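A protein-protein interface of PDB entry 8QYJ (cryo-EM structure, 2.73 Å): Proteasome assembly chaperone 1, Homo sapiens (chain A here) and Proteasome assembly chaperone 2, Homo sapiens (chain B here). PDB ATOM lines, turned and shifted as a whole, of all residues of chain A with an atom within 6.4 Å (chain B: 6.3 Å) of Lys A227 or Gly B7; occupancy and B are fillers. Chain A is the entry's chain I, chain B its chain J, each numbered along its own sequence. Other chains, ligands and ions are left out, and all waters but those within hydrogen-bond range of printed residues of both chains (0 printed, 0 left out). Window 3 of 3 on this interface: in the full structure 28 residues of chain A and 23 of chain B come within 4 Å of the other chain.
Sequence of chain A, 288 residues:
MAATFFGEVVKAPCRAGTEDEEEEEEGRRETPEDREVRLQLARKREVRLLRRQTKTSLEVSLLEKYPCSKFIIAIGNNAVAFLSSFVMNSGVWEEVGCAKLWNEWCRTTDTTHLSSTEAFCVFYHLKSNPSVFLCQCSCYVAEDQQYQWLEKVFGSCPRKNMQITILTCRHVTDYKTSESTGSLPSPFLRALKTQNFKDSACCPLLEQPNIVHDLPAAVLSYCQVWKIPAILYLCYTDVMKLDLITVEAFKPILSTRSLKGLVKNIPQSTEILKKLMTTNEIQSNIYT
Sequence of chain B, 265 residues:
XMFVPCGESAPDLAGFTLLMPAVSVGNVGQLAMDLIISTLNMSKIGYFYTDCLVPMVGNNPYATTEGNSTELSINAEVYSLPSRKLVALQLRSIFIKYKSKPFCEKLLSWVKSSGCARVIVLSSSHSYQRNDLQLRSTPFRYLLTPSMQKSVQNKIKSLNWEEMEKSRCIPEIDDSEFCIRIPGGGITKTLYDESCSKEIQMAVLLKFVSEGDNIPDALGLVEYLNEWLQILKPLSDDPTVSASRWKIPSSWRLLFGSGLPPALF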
ATOM      1  N   ARG A 159       3.091   1.367 -31.947  1.00  0.00           N
ATOM      2  CA  ARG A 159       3.901   2.494 -31.515  1.00  0.00           C
ATOM      3  C   ARG A 159       3.128   3.321 -30.499  1.00  0.00           C
ATOM      4  O   ARG A 159       1.896   3.290 -30.446  1.00  0.00           O
ATOM      5  CB  ARG A 159       4.321   3.373 -32.701  1.00  0.00           C
ATOM      6  CG  ARG A 159       3.237   4.322 -33.183  1.00  0.00           C
ATOM      7  CD  ARG A 159       3.683   5.092 -34.413  1.00  0.00           C
ATOM      8  NE  ARG A 159       3.898   4.213 -35.555  1.00  0.00           N
ATOM      9  CZ  ARG A 159       3.288   4.342 -36.725  1.00  0.00           C
ATOM     10  NH1 ARG A 159       2.413   5.309 -36.947  1.00  0.00           N
ATOM     11  NH2 ARG A 159       3.564   3.478 -37.698  1.00  0.00           N
ATOM     12  N   LYS A 160       3.871   4.059 -29.682  1.00  0.00           N
ATOM     13  CA  LYS A 160       3.299   4.923 -28.666  1.00  0.00           C
ATOM     14  C   LYS A 160       3.171   6.344 -29.213  1.00  0.00           C
ATOM     15  O   LYS A 160       3.401   6.599 -30.399  1.00  0.00           O
ATOM     16  CB  LYS A 160       4.152   4.872 -27.397  1.00  0.00           C
ATOM     17  CG  LYS A 160       4.598   3.473 -27.007  1.00  0.00           C
ATOM     18  CD  LYS A 160       3.514   2.744 -26.231  1.00  0.00           C
ATOM     19  CE  LYS A 160       3.624   1.240 -26.412  1.00  0.00           C
ATOM     20  NZ  LYS A 160       2.916   0.776 -27.638  1.00  0.00           N
ATOM     21  N   GLN A 195      -6.408   2.451 -19.557  1.00  0.00           N
ATOM     22  CA  GLN A 195      -5.795   2.679 -18.255  1.00  0.00           C
ATOM     23  C   GLN A 195      -4.699   3.737 -18.274  1.00  0.00           C
ATOM     24  O   GLN A 195      -4.239   4.140 -17.201  1.00  0.00           O
ATOM     25  CB  GLN A 195      -5.244   1.360 -17.699  1.00  0.00           C
ATOM     26  CG  GLN A 195      -4.130   0.714 -18.515  1.00  0.00           C
ATOM     27  CD  GLN A 195      -2.757   1.274 -18.195  1.00  0.00           C
ATOM     28  OE1 GLN A 195      -2.499   1.710 -17.074  1.00  0.00           O
ATOM     29  NE2 GLN A 195      -1.867   1.261 -19.180  1.00  0.00           N
ATOM     30  N   ASN A 196      -4.272   4.201 -19.449  1.00  0.00           N
ATOM     31  CA  ASN A 196      -3.238   5.225 -19.546  1.00  0.00           C
ATOM     32  C   ASN A 196      -3.752   6.479 -20.249  1.00  0.00           C
ATOM     33  O   ASN A 196      -2.983   7.200 -20.887  1.00  0.00           O
ATOM     34  CB  ASN A 196      -1.994   4.682 -20.247  1.00  0.00           C
ATOM     35  CG  ASN A 196      -2.320   3.943 -21.525  1.00  0.00           C
ATOM     36  OD1 ASN A 196      -3.478   3.626 -21.795  1.00  0.00           O
ATOM     37  ND2 ASN A 196      -1.296   3.659 -22.320  1.00  0.00           N
ATOM     38  N   TYR A 222      -7.753  -3.467 -28.739  1.00  0.00           N
ATOM     39  CA  TYR A 222      -6.405  -3.394 -29.292  1.00  0.00           C
ATOM     40  C   TYR A 222      -5.579  -2.337 -28.567  1.00  0.00           C
ATOM     41  O   TYR A 222      -4.430  -2.586 -28.175  1.00  0.00           O
ATOM     42  CB  TYR A 222      -6.483  -3.098 -30.792  1.00  0.00           C
ATOM     43  CG  TYR A 222      -5.149  -2.977 -31.496  1.00  0.00           C
ATOM     44  CD1 TYR A 222      -4.468  -1.766 -31.537  1.00  0.00           C
ATOM     45  CD2 TYR A 222      -4.580  -4.068 -32.139  1.00  0.00           C
ATOM     46  CE1 TYR A 222      -3.254  -1.652 -32.182  1.00  0.00           C
ATOM     47  CE2 TYR A 222      -3.367  -3.960 -32.789  1.00  0.00           C
ATOM     48  CZ  TYR A 222      -2.708  -2.751 -32.807  1.00  0.00           C
ATOM     49  OH  TYR A 222      -1.500  -2.638 -33.452  1.00  0.00           O
ATOM     50  N   CYS A 223      -6.162  -1.153 -28.364  1.00  0.00           N
ATOM     51  CA  CYS A 223      -5.439  -0.077 -27.692  1.00  0.00           C
ATOM     52  C   CYS A 223      -5.113  -0.440 -26.248  1.00  0.00           C
ATOM     53  O   CYS A 223      -4.019  -0.142 -25.757  1.00  0.00           O
ATOM     54  CB  CYS A 223      -6.249   1.216 -27.752  1.00  0.00           C
ATOM     55  SG  CYS A 223      -6.411   1.906 -29.409  1.00  0.00           S
ATOM     56  N   GLN A 224      -6.056  -1.074 -25.546  1.00  0.00           N
ATOM     57  CA  GLN A 224      -5.813  -1.461 -24.160  1.00  0.00           C
ATOM     58  C   GLN A 224      -4.729  -2.526 -24.060  1.00  0.00           C
ATOM     59  O   GLN A 224      -3.873  -2.466 -23.170  1.00  0.00           O
ATOM     60  CB  GLN A 224      -7.112  -1.953 -23.519  1.00  0.00           C
ATOM     61  CG  GLN A 224      -6.933  -2.626 -22.166  1.00  0.00           C
ATOM     62  CD  GLN A 224      -6.651  -1.640 -21.048  1.00  0.00           C
ATOM     63  OE1 GLN A 224      -7.548  -1.264 -20.298  1.00  0.00           O
ATOM     64  NE2 GLN A 224      -5.398  -1.224 -20.928  1.00  0.00           N
ATOM     65  N   VAL A 225      -4.749  -3.510 -24.961  1.00  0.00           N
ATOM     66  CA  VAL A 225      -3.755  -4.576 -24.917  1.00  0.00           C
ATOM     67  C   VAL A 225      -2.367  -4.034 -25.235  1.00  0.00           C
ATOM     68  O   VAL A 225      -1.386  -4.377 -24.564  1.00  0.00           O
ATOM     69  CB  VAL A 225      -4.151  -5.718 -25.871  1.00  0.00           C
ATOM     70  CG1 VAL A 225      -2.999  -6.690 -26.042  1.00  0.00           C
ATOM     71  CG2 VAL A 225      -5.377  -6.442 -25.347  1.00  0.00           C
ATOM     72  N   TRP A 226      -2.256  -3.174 -26.249  1.00  0.00           N
ATOM     73  CA  TRP A 226      -0.952  -2.712 -26.706  1.00  0.00           C
ATOM     74  C   TRP A 226      -0.539  -1.381 -26.084  1.00  0.00           C
ATOM     75  O   TRP A 226       0.402  -0.745 -26.571  1.00  0.00           O
ATOM     76  CB  TRP A 226      -0.931  -2.625 -28.231  1.00  0.00           C
ATOM     77  CG  TRP A 226      -1.082  -3.967 -28.881  1.00  0.00           C
ATOM     78  CD1 TRP A 226      -2.078  -4.360 -29.723  1.00  0.00           C
ATOM     79  CD2 TRP A 226      -0.222  -5.103 -28.720  1.00  0.00           C
ATOM     80  NE1 TRP A 226      -1.888  -5.665 -30.106  1.00  0.00           N
ATOM     81  CE2 TRP A 226      -0.756  -6.144 -29.503  1.00  0.00           C
ATOM     82  CE3 TRP A 226       0.950  -5.339 -27.994  1.00  0.00           C
ATOM     83  CZ2 TRP A 226      -0.159  -7.400 -29.581  1.00  0.00           C
ATOM     84  CZ3 TRP A 226       1.539  -6.586 -28.073  1.00  0.00           C
ATOM     85  CH2 TRP A 226       0.986  -7.600 -28.861  1.00  0.00           C
ATOM     86  N   LYS A 227      -1.223  -0.953 -25.021  1.00  0.00           N
ATOM     87  CA  LYS A 227      -0.828   0.207 -24.219  1.00  0.00           C
ATOM     88  C   LYS A 227      -0.780   1.486 -25.061  1.00  0.00           C
ATOM     89  O   LYS A 227       0.259   2.132 -25.208  1.00  0.00           O
ATOM     90  CB  LYS A 227       0.516  -0.044 -23.526  1.00  0.00           C
ATOM     91  CG  LYS A 227       0.471  -1.120 -22.455  1.00  0.00           C
ATOM     92  CD  LYS A 227       1.856  -1.400 -21.899  1.00  0.00           C
ATOM     93  CE  LYS A 227       1.817  -2.493 -20.847  1.00  0.00           C
ATOM     94  NZ  LYS A 227       1.652  -3.842 -21.455  1.00  0.00           N
ATOM     95  N   ILE A 228      -1.936   1.845 -25.609  1.00  0.00           N
ATOM     96  CA  ILE A 228      -2.106   3.060 -26.394  1.00  0.00           C
ATOM     97  C   ILE A 228      -3.243   3.857 -25.772  1.00  0.00           C
ATOM     98  O   ILE A 228      -4.322   3.305 -25.554  1.00  0.00           O
ATOM     99  CB  ILE A 228      -2.410   2.768 -27.875  1.00  0.00           C
ATOM    100  CG1 ILE A 228      -1.271   1.971 -28.510  1.00  0.00           C
ATOM    101  CG2 ILE A 228      -2.645   4.061 -28.637  1.00  0.00           C
ATOM    102  CD1 ILE A 228      -1.674   1.230 -29.764  1.00  0.00           C
ATOM    103  N   PRO A 229      -3.048   5.136 -25.452  1.00  0.00           N
ATOM    104  CA  PRO A 229      -4.156   5.935 -24.915  1.00  0.00           C
ATOM    105  C   PRO A 229      -5.289   6.054 -25.924  1.00  0.00           C
ATOM    106  O   PRO A 229      -5.064   6.284 -27.113  1.00  0.00           O
ATOM    107  CB  PRO A 229      -3.510   7.296 -24.628  1.00  0.00           C
ATOM    108  CG  PRO A 229      -2.040   7.028 -24.576  1.00  0.00           C
ATOM    109  CD  PRO A 229      -1.797   5.906 -25.530  1.00  0.00           C
ATOM    110  N   VAL B   4      -0.095 -11.552 -23.000  1.00  0.00           N
ATOM    111  CA  VAL B   4       0.448 -10.202 -22.899  1.00  0.00           C
ATOM    112  C   VAL B   4       0.327  -9.759 -21.446  1.00  0.00           C
ATOM    113  O   VAL B   4      -0.793  -9.589 -20.948  1.00  0.00           O
ATOM    114  CB  VAL B   4      -0.279  -9.225 -23.836  1.00  0.00           C
ATOM    115  CG1 VAL B   4       0.253  -7.817 -23.648  1.00  0.00           C
ATOM    116  CG2 VAL B   4      -0.132  -9.667 -25.282  1.00  0.00           C
ATOM    117  N   PRO B   5       1.433  -9.575 -20.729  1.00  0.00           N
ATOM    118  CA  PRO B   5       1.339  -9.166 -19.324  1.00  0.00           C
ATOM    119  C   PRO B   5       0.801  -7.753 -19.177  1.00  0.00           C
ATOM    120  O   PRO B   5       0.958  -6.904 -20.058  1.00  0.00           O
ATOM    121  CB  PRO B   5       2.787  -9.261 -18.831  1.00  0.00           C
ATOM    122  CG  PRO B   5       3.612  -9.104 -20.060  1.00  0.00           C
ATOM    123  CD  PRO B   5       2.828  -9.742 -21.169  1.00  0.00           C
ATOM    124  N   CYS B   6       0.152  -7.508 -18.037  1.00  0.00           N
ATOM    125  CA  CYS B   6      -0.347  -6.168 -17.745  1.00  0.00           C
ATOM    126  C   CYS B   6       0.785  -5.212 -17.398  1.00  0.00           C
ATOM    127  O   CYS B   6       0.653  -3.998 -17.598  1.00  0.00           O
ATOM    128  CB  CYS B   6      -1.362  -6.220 -16.603  1.00  0.00           C
ATOM    129  SG  CYS B   6      -3.053  -6.576 -17.120  1.00  0.00           S
ATOM    130  N   GLY B   7       1.891  -5.728 -16.881  1.00  0.00           N
ATOM    131  CA  GLY B   7       3.045  -4.929 -16.508  1.00  0.00           C
ATOM    132  C   GLY B   7       4.137  -4.982 -17.553  1.00  0.00           C
ATOM    133  O   GLY B   7       3.871  -4.980 -18.761  1.00  0.00           O
ATOM    134  N   GLU B   8       5.384  -5.032 -17.087  1.00  0.00           N
ATOM    135  CA  GLU B   8       6.536  -5.052 -17.980  1.00  0.00           C
ATOM    136  C   GLU B   8       6.971  -6.472 -18.327  1.00  0.00           C
ATOM    137  O   GLU B   8       7.193  -6.786 -19.500  1.00  0.00           O
ATOM    138  CB  GLU B   8       7.700  -4.283 -17.348  1.00  0.00           C
ATOM    139  CG  GLU B   8       7.445  -2.793 -17.191  1.00  0.00           C
ATOM    140  CD  GLU B   8       7.336  -2.077 -18.522  1.00  0.00           C
ATOM    141  OE1 GLU B   8       8.002  -2.506 -19.487  1.00  0.00           O
ATOM    142  OE2 GLU B   8       6.582  -1.084 -18.604  1.00  0.00           O
ATOM    143  N   SER B   9       7.094  -7.338 -17.324  1.00  0.00           N
ATOM    144  CA  SER B   9       7.553  -8.706 -17.520  1.00  0.00           C
ATOM    145  C   SER B   9       6.528  -9.678 -16.957  1.00  0.00           C
ATOM    146  O   SER B   9       5.964  -9.448 -15.884  1.00  0.00           O
ATOM    147  CB  SER B   9       8.915  -8.938 -16.853  1.00  0.00           C
ATOM    148  OG  SER B   9       8.826  -8.786 -15.447  1.00  0.00           O
ATOM    149  N   ALA B  10       6.293 -10.763 -17.690  1.00  0.00           N
ATOM    150  CA  ALA B  10       5.351 -11.774 -17.243  1.00  0.00           C
ATOM    151  C   ALA B  10       5.914 -12.540 -16.046  1.00  0.00           C
ATOM    152  O   ALA B  10       7.124 -12.758 -15.951  1.00  0.00           O
ATOM    153  CB  ALA B  10       5.032 -12.744 -18.377  1.00  0.00           C
ATOM    154  N   ILE B  45      -3.374 -10.228 -14.086  1.00  0.00           N
ATOM    155  CA  ILE B  45      -1.940 -10.288 -14.349  1.00  0.00           C
ATOM    156  C   ILE B  45      -1.645 -10.158 -15.839  1.00  0.00           C
ATOM    157  O   ILE B  45      -0.492  -9.939 -16.231  1.00  0.00           O
ATOM    158  CB  ILE B  45      -1.321 -11.582 -13.786  1.00  0.00           C
ATOM    159  CG1 ILE B  45      -2.039 -12.813 -14.341  1.00  0.00           C
ATOM    160  CG2 ILE B  45      -1.346 -11.574 -12.265  1.00  0.00           C
ATOM    161  CD1 ILE B  45      -1.153 -14.031 -14.452  1.00  0.00           C
ATOM    162  N   TYR B  47      -3.508 -10.531 -20.223  1.00  0.00           N
ATOM    163  CA  TYR B  47      -4.570 -10.840 -21.168  1.00  0.00           C
ATOM    164  C   TYR B  47      -4.126 -11.976 -22.078  1.00  0.00           C
ATOM    165  O   TYR B  47      -2.933 -12.223 -22.263  1.00  0.00           O
ATOM    166  CB  TYR B  47      -4.951  -9.624 -22.031  1.00  0.00           C
ATOM    167  CG  TYR B  47      -4.969  -8.301 -21.299  1.00  0.00           C
ATOM    168  CD1 TYR B  47      -6.119  -7.849 -20.669  1.00  0.00           C
ATOM    169  CD2 TYR B  47      -3.839  -7.496 -21.253  1.00  0.00           C
ATOM    170  CE1 TYR B  47      -6.141  -6.641 -20.005  1.00  0.00           C
ATOM    171  CE2 TYR B  47      -3.852  -6.287 -20.592  1.00  0.00           C
ATOM    172  CZ  TYR B  47      -5.005  -5.864 -19.969  1.00  0.00           C
ATOM    173  OH  TYR B  47      -5.021  -4.658 -19.308  1.00  0.00           O
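Of the 9 printed residues of chain B, 5 touch a printed residue of chain A. Printed residues of chain B that touch a printed residue of chain A: Val B4, Pro B5, Cys B6, Gly B7 and Tyr B47. Of the 12 printed residues of chain A, 3 touch a printed residue of chain B. Among the printed residues, no Asp or Glu carboxylate lies within 4 Å of a Lys or Arg side-chain nitrogen of the other chain.
Lys A227 touches three residues of chain B. Of chain A, only Lys A227 comes within 4 Å of Gly B7. Of the printed residues of chain A, Pro B5 touches Lys A227. Printed residues of chain B within 4 Å of Val A225: Val B4 (3.9 Å). Of the printed residues of chain A, Tyr B47 touches Gln A224. Asn A196 touches none of the printed residues of chain B. Cys A223 touches none of the printed residues of chain B. The nearest printed residue of chain A that does not touch Cys B6 is Gln A195 (6.0 Å).
Tyr B47 touches Gln A224 (OH to NE2, 3.8 Å). Val A225 touches Val B4. Lys A227 touches Cys B6. NZ of Lys A227 touches O of Gly B7 (3.7 Å).
The backbone carbonyl oxygen (O) of Val B4 sits at hydrogen-bond distance from the backbone NH (N) of Tyr B47 (3.0 Å). The backbone NH of Cys B6 is in hydrogen-bond range of the backbone carbonyl oxygen of Ile B45 (3.1 Å). The side-chain sulfur (SG) of Cys B6 lies within hydrogen-bond range of the side-chain hydroxyl (OH) of Tyr B47 (3.5 Å).
O of Pro B5 is in hydrogen-bond range of NZ of Lys A227 (3.4 Å).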
